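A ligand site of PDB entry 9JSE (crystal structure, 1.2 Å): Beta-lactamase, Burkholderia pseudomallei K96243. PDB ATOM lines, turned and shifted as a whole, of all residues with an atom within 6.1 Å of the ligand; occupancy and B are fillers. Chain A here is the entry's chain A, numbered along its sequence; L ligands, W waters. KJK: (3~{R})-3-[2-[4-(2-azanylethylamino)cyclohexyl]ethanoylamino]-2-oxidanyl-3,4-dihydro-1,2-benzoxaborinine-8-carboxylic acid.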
ATOM      1  N   PHE A  43      23.450 -10.888  -8.609  1.00  0.00           N
ATOM      2  CA  PHE A  43      22.743  -9.773  -9.244  1.00  0.00           C
ATOM      3  C   PHE A  43      23.554  -8.476  -9.278  1.00  0.00           C
ATOM      4  O   PHE A  43      23.252  -7.601 -10.101  1.00  0.00           O
ATOM      5  CB  PHE A  43      21.341  -9.574  -8.649  1.00  0.00           C
ATOM      6  CG  PHE A  43      21.255  -9.527  -7.144  1.00  0.00           C
ATOM      7  CD1 PHE A  43      22.065  -8.702  -6.387  1.00  0.00           C
ATOM      8  CD2 PHE A  43      20.318 -10.300  -6.484  1.00  0.00           C
ATOM      9  CE1 PHE A  43      21.958  -8.654  -5.008  1.00  0.00           C
ATOM     10  CE2 PHE A  43      20.196 -10.239  -5.109  1.00  0.00           C
ATOM     11  CZ  PHE A  43      21.008  -9.419  -4.373  1.00  0.00           C
ATOM     12  N   CYS A  44      24.588  -8.338  -8.445  1.00  0.00           N
ATOM     13  CA  CYS A  44      25.420  -7.136  -8.405  1.00  0.00           C
ATOM     14  C   CYS A  44      24.537  -5.895  -8.344  1.00  0.00           C
ATOM     15  O   CYS A  44      23.519  -5.885  -7.628  1.00  0.00           O
ATOM     16  CB  CYS A  44      26.423  -7.167  -9.557  1.00  0.00           C
ATOM     17  SG  CYS A  44      27.540  -8.594  -9.424  1.00  0.00           S
ATOM     18  N   SER A  45      24.859  -4.852  -9.103  1.00  0.00           N
ATOM     19  CA  SER A  45      24.181  -3.590  -8.881  1.00  0.00           C
ATOM     20  C   SER A  45      22.752  -3.597  -9.406  1.00  0.00           C
ATOM     21  O   SER A  45      22.034  -2.617  -9.186  1.00  0.00           O
ATOM     22  CB  SER A  45      24.965  -2.439  -9.512  1.00  0.00           C
ATOM     23  OG  SER A  45      26.188  -2.125  -8.831  1.00  0.00           O
ATOM     24  N   THR A  46      22.294  -4.658 -10.077  1.00  0.00           N
ATOM     25  CA  THR A  46      20.888  -4.678 -10.470  1.00  0.00           C
ATOM     26  C   THR A  46      19.991  -4.671  -9.234  1.00  0.00           C
ATOM     27  O   THR A  46      18.820  -4.283  -9.334  1.00  0.00           O
ATOM     28  CB  THR A  46      20.510  -5.837 -11.412  1.00  0.00           C
ATOM     29  OG1 THR A  46      20.585  -7.094 -10.722  1.00  0.00           O
ATOM     30  CG2 THR A  46      21.388  -5.840 -12.668  1.00  0.00           C
ATOM     31  N   LYS A  48      20.050  -2.581  -7.001  1.00  0.00           N
ATOM     32  CA  LYS A  48      19.712  -1.190  -6.681  1.00  0.00           C
ATOM     33  C   LYS A  48      18.304  -0.856  -7.139  1.00  0.00           C
ATOM     34  O   LYS A  48      17.666   0.026  -6.559  1.00  0.00           O
ATOM     35  CB  LYS A  48      20.773  -0.267  -7.271  1.00  0.00           C
ATOM     36  CG  LYS A  48      22.102  -0.338  -6.508  1.00  0.00           C
ATOM     37  CD  LYS A  48      23.277   0.206  -7.295  1.00  0.00           C
ATOM     38  CE  LYS A  48      24.553   0.131  -6.445  1.00  0.00           C
ATOM     39  NZ  LYS A  48      25.830   0.115  -7.200  1.00  0.00           N
ATOM     40  N   ARG A  79      34.494   3.001  -3.318  1.00  0.00           N
ATOM     41  CA  ARG A  79      34.763   3.082  -4.743  1.00  0.00           C
ATOM     42  C   ARG A  79      33.458   3.044  -5.543  1.00  0.00           C
ATOM     43  O   ARG A  79      32.449   2.496  -5.105  1.00  0.00           O
ATOM     44  CB  ARG A  79      35.701   1.971  -5.215  1.00  0.00           C
ATOM     45  CG  ARG A  79      36.946   1.777  -4.382  1.00  0.00           C
ATOM     46  CD  ARG A  79      38.045   1.060  -5.165  1.00  0.00           C
ATOM     47  NE  ARG A  79      38.111   1.441  -6.573  1.00  0.00           N
ATOM     48  NH1 ARG A  79      39.827  -0.008  -7.079  1.00  0.00           N
ATOM     49  N   TYR A  80      33.522   3.610  -6.739  1.00  0.00           N
ATOM     50  CA  TYR A  80      32.410   3.614  -7.684  1.00  0.00           C
ATOM     51  C   TYR A  80      31.228   4.376  -7.110  1.00  0.00           C
ATOM     52  O   TYR A  80      30.095   3.889  -7.092  1.00  0.00           O
ATOM     53  CB  TYR A  80      32.057   2.200  -8.161  1.00  0.00           C
ATOM     54  CG  TYR A  80      33.264   1.417  -8.587  1.00  0.00           C
ATOM     55  CD1 TYR A  80      33.897   1.691  -9.790  1.00  0.00           C
ATOM     56  CD2 TYR A  80      33.813   0.419  -7.778  1.00  0.00           C
ATOM     57  CE1 TYR A  80      35.023   0.997 -10.177  1.00  0.00           C
ATOM     58  CE2 TYR A  80      34.928  -0.270  -8.154  1.00  0.00           C
ATOM     59  CZ  TYR A  80      35.531   0.017  -9.357  1.00  0.00           C
ATOM     60  OH  TYR A  80      36.642  -0.664  -9.747  1.00  0.00           O
ATOM     61  N   TYR A 104      23.922   6.160 -12.043  1.00  0.00           N
ATOM     62  CA  TYR A 104      25.380   6.131 -12.076  1.00  0.00           C
ATOM     63  C   TYR A 104      25.918   4.934 -11.313  1.00  0.00           C
ATOM     64  O   TYR A 104      27.140   4.801 -11.188  1.00  0.00           O
ATOM     65  CB  TYR A 104      25.940   7.418 -11.469  1.00  0.00           C
ATOM     66  CG  TYR A 104      25.651   8.662 -12.263  1.00  0.00           C
ATOM     67  CD1 TYR A 104      24.455   9.345 -12.114  1.00  0.00           C
ATOM     68  CD2 TYR A 104      26.569   9.179 -13.183  1.00  0.00           C
ATOM     69  CE1 TYR A 104      24.173  10.477 -12.831  1.00  0.00           C
ATOM     70  CE2 TYR A 104      26.285  10.324 -13.908  1.00  0.00           C
ATOM     71  CZ  TYR A 104      25.071  10.960 -13.738  1.00  0.00           C
ATOM     72  OH  TYR A 104      24.776  12.098 -14.444  1.00  0.00           O
ATOM     73  N   SER A 105      25.058   4.065 -10.806  1.00  0.00           N
ATOM     74  CA  SER A 105      25.442   2.898 -10.022  1.00  0.00           C
ATOM     75  C   SER A 105      26.248   3.269  -8.769  1.00  0.00           C
ATOM     76  O   SER A 105      27.074   2.492  -8.305  1.00  0.00           O
ATOM     77  CB  SER A 105      26.117   1.814 -10.848  1.00  0.00           C
ATOM     78  OG  SER A 105      25.777   0.581 -10.234  1.00  0.00           O
ATOM     79  N   ASN A 107      27.780   3.452  -5.412  1.00  0.00           N
ATOM     80  CA  ASN A 107      27.802   2.450  -4.337  1.00  0.00           C
ATOM     81  C   ASN A 107      27.569   3.068  -2.966  1.00  0.00           C
ATOM     82  O   ASN A 107      26.858   2.466  -2.143  1.00  0.00           O
ATOM     83  CB  ASN A 107      29.109   1.660  -4.332  1.00  0.00           C
ATOM     84  CG  ASN A 107      29.111   0.516  -5.297  1.00  0.00           C
ATOM     85  OD1 ASN A 107      28.085   0.037  -5.728  1.00  0.00           O
ATOM     86  ND2 ASN A 107      30.292   0.013  -5.573  1.00  0.00           N
ATOM     87  N   GLU A 141      27.418  -2.867  -0.103  1.00  0.00           N
ATOM     88  CA  GLU A 141      28.469  -2.568  -1.071  1.00  0.00           C
ATOM     89  C   GLU A 141      29.812  -2.398  -0.347  1.00  0.00           C
ATOM     90  O   GLU A 141      29.845  -1.806   0.733  1.00  0.00           O
ATOM     91  CB  GLU A 141      28.182  -1.281  -1.831  1.00  0.00           C
ATOM     92  CG  GLU A 141      26.921  -1.298  -2.631  1.00  0.00           C
ATOM     93  CD  GLU A 141      27.017  -2.176  -3.861  1.00  0.00           C
ATOM     94  OE1 GLU A 141      28.092  -2.763  -4.108  1.00  0.00           O
ATOM     95  OE2 GLU A 141      25.989  -2.259  -4.585  1.00  0.00           O
ATOM     96  N   PRO A 142      30.914  -2.853  -0.940  1.00  0.00           N
ATOM     97  CA  PRO A 142      31.006  -3.479  -2.259  1.00  0.00           C
ATOM     98  C   PRO A 142      30.979  -5.010  -2.249  1.00  0.00           C
ATOM     99  O   PRO A 142      31.041  -5.632  -3.324  1.00  0.00           O
ATOM    100  CB  PRO A 142      32.394  -3.020  -2.741  1.00  0.00           C
ATOM    101  CG  PRO A 142      33.206  -3.002  -1.494  1.00  0.00           C
ATOM    102  CD  PRO A 142      32.249  -2.595  -0.362  1.00  0.00           C
ATOM    103  N   ASN A 145      29.217  -7.844  -4.561  1.00  0.00           N
ATOM    104  CA  ASN A 145      29.599  -8.104  -5.943  1.00  0.00           C
ATOM    105  C   ASN A 145      30.649  -9.200  -6.120  1.00  0.00           C
ATOM    106  O   ASN A 145      31.228  -9.316  -7.209  1.00  0.00           O
ATOM    107  CB  ASN A 145      30.125  -6.804  -6.585  1.00  0.00           C
ATOM    108  CG  ASN A 145      29.120  -5.689  -6.526  1.00  0.00           C
ATOM    109  OD1 ASN A 145      28.129  -5.687  -7.263  1.00  0.00           O
ATOM    110  ND2 ASN A 145      29.384  -4.708  -5.675  1.00  0.00           N
ATOM    111  N   THR A 191      24.528   4.221 -17.450  1.00  0.00           N
ATOM    112  CA  THR A 191      25.546   3.174 -17.492  1.00  0.00           C
ATOM    113  C   THR A 191      25.237   2.030 -18.450  1.00  0.00           C
ATOM    114  O   THR A 191      26.009   1.067 -18.504  1.00  0.00           O
ATOM    115  CB  THR A 191      25.745   2.582 -16.098  1.00  0.00           C
ATOM    116  OG1 THR A 191      24.520   1.919 -15.727  1.00  0.00           O
ATOM    117  CG2 THR A 191      26.071   3.648 -15.051  1.00  0.00           C
ATOM    118  N   ARG A 195      24.585  -2.148 -23.495  1.00  0.00           N
ATOM    119  CA  ARG A 195      23.965  -3.388 -23.020  1.00  0.00           C
ATOM    120  C   ARG A 195      22.585  -3.528 -23.657  1.00  0.00           C
ATOM    121  O   ARG A 195      22.502  -3.566 -24.886  1.00  0.00           O
ATOM    122  CB  ARG A 195      24.082  -3.475 -21.499  1.00  0.00           C
ATOM    123  CG  ARG A 195      25.568  -3.492 -21.069  1.00  0.00           C
ATOM    124  CD  ARG A 195      25.732  -3.758 -19.597  1.00  0.00           C
ATOM    125  NE  ARG A 195      27.120  -4.057 -19.261  1.00  0.00           N
ATOM    126  CZ  ARG A 195      27.567  -4.233 -18.021  1.00  0.00           C
ATOM    127  NH1 ARG A 195      26.729  -4.448 -17.027  1.00  0.00           N
ATOM    128  NH2 ARG A 195      28.885  -4.253 -17.785  1.00  0.00           N
ATOM    129  N   LYS A 209      18.659  -1.051 -15.394  1.00  0.00           N
ATOM    130  CA  LYS A 209      19.702  -0.975 -14.383  1.00  0.00           C
ATOM    131  C   LYS A 209      20.744  -2.062 -14.659  1.00  0.00           C
ATOM    132  O   LYS A 209      20.403  -3.236 -14.745  1.00  0.00           O
ATOM    133  CB  LYS A 209      19.154  -1.200 -12.981  1.00  0.00           C
ATOM    134  CG  LYS A 209      20.174  -1.085 -11.856  1.00  0.00           C
ATOM    135  CD  LYS A 209      20.815   0.295 -11.730  1.00  0.00           C
ATOM    136  CE  LYS A 209      22.108   0.292 -10.915  1.00  0.00           C
ATOM    137  NZ  LYS A 209      23.287   0.090 -11.809  1.00  0.00           N
ATOM    138  N   THR A 210      21.982  -1.662 -14.805  1.00  0.00           N
ATOM    139  CA  THR A 210      23.082  -2.564 -15.051  1.00  0.00           C
ATOM    140  C   THR A 210      23.671  -3.085 -13.738  1.00  0.00           C
ATOM    141  O   THR A 210      23.414  -2.575 -12.642  1.00  0.00           O
ATOM    142  CB  THR A 210      24.188  -1.805 -15.793  1.00  0.00           C
ATOM    143  OG1 THR A 210      24.498  -0.611 -15.092  1.00  0.00           O
ATOM    144  CG2 THR A 210      23.763  -1.432 -17.191  1.00  0.00           C
ATOM    145  N   GLY A 211      24.534  -4.087 -13.863  1.00  0.00           N
ATOM    146  CA  GLY A 211      25.430  -4.461 -12.787  1.00  0.00           C
ATOM    147  C   GLY A 211      26.706  -5.020 -13.363  1.00  0.00           C
ATOM    148  O   GLY A 211      26.696  -5.644 -14.431  1.00  0.00           O
ATOM    149  N   THR A 212      27.802  -4.812 -12.647  1.00  0.00           N
ATOM    150  CA  THR A 212      29.075  -5.406 -13.011  1.00  0.00           C
ATOM    151  C   THR A 212      29.725  -5.893 -11.722  1.00  0.00           C
ATOM    152  O   THR A 212      29.682  -5.204 -10.703  1.00  0.00           O
ATOM    153  CB  THR A 212      29.969  -4.357 -13.681  1.00  0.00           C
ATOM    154  OG1 THR A 212      29.344  -3.895 -14.890  1.00  0.00           O
ATOM    155  CG2 THR A 212      31.317  -4.956 -14.038  1.00  0.00           C
ATOM    156  N   GLY A 213      30.288  -7.095 -11.760  1.00  0.00           N
ATOM    157  CA  GLY A 213      30.904  -7.653 -10.575  1.00  0.00           C
ATOM    158  C   GLY A 213      32.165  -8.414 -10.873  1.00  0.00           C
ATOM    159  O   GLY A 213      32.674  -8.372 -12.003  1.00  0.00           O
ATOM    160  N   ASP A 214      32.676  -9.102  -9.870  1.00  0.00           N
ATOM    161  CA  ASP A 214      33.836  -9.960 -10.049  1.00  0.00           C
ATOM    162  C   ASP A 214      33.472 -11.140 -10.959  1.00  0.00           C
ATOM    163  O   ASP A 214      32.325 -11.301 -11.369  1.00  0.00           O
ATOM    164  CB  ASP A 214      34.405 -10.418  -8.709  1.00  0.00           C
ATOM    165  CG  ASP A 214      34.893  -9.261  -7.829  1.00  0.00           C
ATOM    166  OD1 ASP A 214      35.264  -8.191  -8.378  1.00  0.00           O
ATOM    167  OD2 ASP A 214      35.113  -9.490  -6.619  1.00  0.00           O
ATOM    168  N   ASN A 219      25.576  -7.716 -16.012  1.00  0.00           N
ATOM    169  CA  ASN A 219      24.137  -7.856 -15.992  1.00  0.00           C
ATOM    170  C   ASN A 219      23.441  -6.603 -16.474  1.00  0.00           C
ATOM    171  O   ASN A 219      23.985  -5.497 -16.410  1.00  0.00           O
ATOM    172  CB  ASN A 219      23.637  -8.126 -14.563  1.00  0.00           C
ATOM    173  CG  ASN A 219      24.426  -9.196 -13.832  1.00  0.00           C
ATOM    174  OD1 ASN A 219      24.827 -10.198 -14.412  1.00  0.00           O
ATOM    175  ND2 ASN A 219      24.555  -9.047 -12.514  1.00  0.00           N
ATOM    176  N   GLN A 246      37.326 -10.379 -17.778  1.00  0.00           N
ATOM    177  CA  GLN A 246      37.030  -8.965 -17.969  1.00  0.00           C
ATOM    178  C   GLN A 246      35.569  -8.848 -18.369  1.00  0.00           C
ATOM    179  O   GLN A 246      35.153  -9.430 -19.382  1.00  0.00           O
ATOM    180  CB  GLN A 246      37.932  -8.392 -19.061  1.00  0.00           C
ATOM    181  CG  GLN A 246      37.546  -7.012 -19.542  1.00  0.00           C
ATOM    182  CD  GLN A 246      37.601  -6.011 -18.436  1.00  0.00           C
ATOM    183  OE1 GLN A 246      38.640  -5.833 -17.806  1.00  0.00           O
ATOM    184  NE2 GLN A 246      36.481  -5.347 -18.175  1.00  0.00           N
HETATM  185  B07 KJK L   1      27.489  -2.386  -9.662  1.00  0.00           B
HETATM  186  C10 KJK L   1      28.430  -1.064 -11.397  1.00  0.00           C
HETATM  187  C11 KJK L   1      28.493  -1.044 -12.793  1.00  0.00           C
HETATM  188  C12 KJK L   1      27.309  -1.401 -13.613  1.00  0.00           C
HETATM  189  C15 KJK L   1      29.669  -0.623 -13.365  1.00  0.00           C
HETATM  190  C16 KJK L   1      30.751  -0.219 -12.618  1.00  0.00           C
HETATM  191  C17 KJK L   1      30.667  -0.233 -11.221  1.00  0.00           C
HETATM  192  C18 KJK L   1      29.495  -0.664 -10.596  1.00  0.00           C
HETATM  193  C19 KJK L   1      29.313  -0.661  -9.124  1.00  0.00           C
HETATM  194  C20 KJK L   1      28.733  -2.005  -8.680  1.00  0.00           C
HETATM  195  C22 KJK L   1      30.925  -3.079  -8.102  1.00  0.00           C
HETATM  196  C23 KJK L   1      31.957  -4.134  -8.334  1.00  0.00           C
HETATM  197  C24 KJK L   1      33.107  -3.692  -9.209  1.00  0.00           C
HETATM  198  C25 KJK L   1      32.679  -3.101 -10.497  1.00  0.00           C
HETATM  199  C26 KJK L   1      33.889  -2.663 -11.303  1.00  0.00           C
HETATM  200  C27 KJK L   1      34.826  -3.810 -11.682  1.00  0.00           C
HETATM  201  C29 KJK L   1      36.998  -4.354 -12.780  1.00  0.00           C
HETATM  202  C30 KJK L   1      38.269  -3.718 -13.420  1.00  0.00           C
HETATM  203  C32 KJK L   1      35.149  -4.707 -10.483  1.00  0.00           C
HETATM  204  C33 KJK L   1      34.010  -4.906  -9.469  1.00  0.00           C
HETATM  205  N21 KJK L   1      29.812  -3.000  -8.842  1.00  0.00           N
HETATM  206  N28 KJK L   1      36.089  -3.315 -12.296  1.00  0.00           N
HETATM  207  N31 KJK L   1      37.936  -2.852 -14.527  1.00  0.00           N
HETATM  208  O08 KJK L   1      27.365  -3.752 -10.035  1.00  0.00           O
HETATM  209  O09 KJK L   1      27.254  -1.506 -10.789  1.00  0.00           O
HETATM  210  O13 KJK L   1      26.216  -0.826 -13.284  1.00  0.00           O
HETATM  211  O14 KJK L   1      27.449  -2.076 -14.653  1.00  0.00           O
HETATM  212  O34 KJK L   1      31.141  -2.248  -7.150  1.00  0.00           O
HETATM  213  O   HOH W   1      26.369  -3.698  -6.661  1.00  0.00           O
HETATM  214  O   HOH W   2      27.435  -1.089 -17.292  1.00  0.00           O
HETATM  215  O   HOH W   3      35.141  -4.160 -15.219  1.00  0.00           O
HETATM  216  O   HOH W   4      33.522  -2.005  -5.722  1.00  0.00           O
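An oxygen (O34) of the ligand is in hydrogen-bond range of the side-chain amide nitrogen (ND2) of Asn 107 (2.9 Å). The side-chain hydroxyl of Thr 212 sits at hydrogen-bond distance from an oxygen (O14) of the ligand, at 2.6 Å. OG1 of Thr 210 lies within hydrogen-bond range of O13 of the ligand (2.5 Å). An oxygen (O09) of the ligand is in hydrogen-bond range of the side-chain hydroxyl (OG) of Ser 105. An oxygen (O34) of the ligand sits close to the side-chain amide nitrogen of Asn 145 (3.4 Å). The backbone carbonyl oxygen (O) of Thr 212 sits at hydrogen-bond distance from an oxygen (O08) of the ligand (2.8 Å). An oxygen (O13) of the ligand lies within salt-bridge range of the side-chain amino group of Lys 209. The backbone NH (N) of Ser 45 lies close to an oxygen (O08) of the ligand, 2.9 Å away. OG of Ser 45 is bonded to B07 of the ligand, 1.6 Å away. NH1 of Arg 195 is in salt-bridge range of O14 of the ligand, 3.4 Å away. N of Thr 212 lies within hydrogen-bond range of O08 of the ligand (2.9 Å).
ND2 of Asn 145 lies within hydrogen-bond range of O of Pro 142, 3.0 Å away. The side-chain hydroxyl (OG) of Ser 105 sits at hydrogen-bond distance from the side-chain hydroxyl (OG) of Ser 45 (3.1 Å). O of Ser 105 is in hydrogen-bond range of NZ of Lys 48, at 2.9 Å. The side-chain amino group (NZ) of Lys 48 is in hydrogen-bond range of the side-chain hydroxyl (OG) of Ser 45 (2.8 Å). The guanidinium group (NH1) of Arg 195 sits at hydrogen-bond distance from the backbone carbonyl oxygen (O) of Gly 211, at 2.9 Å. The side-chain hydroxyl of Thr 191 lies within hydrogen-bond range of the side-chain hydroxyl of Thr 210. NH1 of Arg 195 is in hydrogen-bond range of O of Asn 219 (3.0 Å). OD1 of Asn 107 lies close to OE1 of Glu 141 (3.2 Å).
Cys 44 touches the ligand. NZ of Lys 48 touches B07 of the ligand (3.9 Å). Tyr 80 touches the ligand (CZ to C26, 3.7 Å). Gly 211 touches the ligand (C to O14, 3.3 Å). Asp 214 touches the ligand (OD1 to C33, 3.7 Å). Hydrophobic or aromatic side chains that line the ligand: Tyr 80. 13 residues have an atom within 4 Å of the ligand: Cys 44, Ser 45, Lys 48, Tyr 80, Ser 105, Asn 107, Asn 145, Arg 195, Lys 209, Thr 210, Gly 211, Thr 212 and Asp 214. The nearest printed residue that does not touch the ligand is Thr 191 (4.05 Å).
Water W2 lies within hydrogen-bond range of an oxygen (O14) of the ligand (2.8 Å), the backbone carbonyl oxygen (O) of Thr 191 (2.9 Å) and the guanidinium group (NH1) of Arg 195 (3.4 Å). Water W3 lies within hydrogen-bond range of a nitrogen (N31) of the ligand (3.2 Å) and the side-chain amide nitrogen of Gln 246 (3.5 Å).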
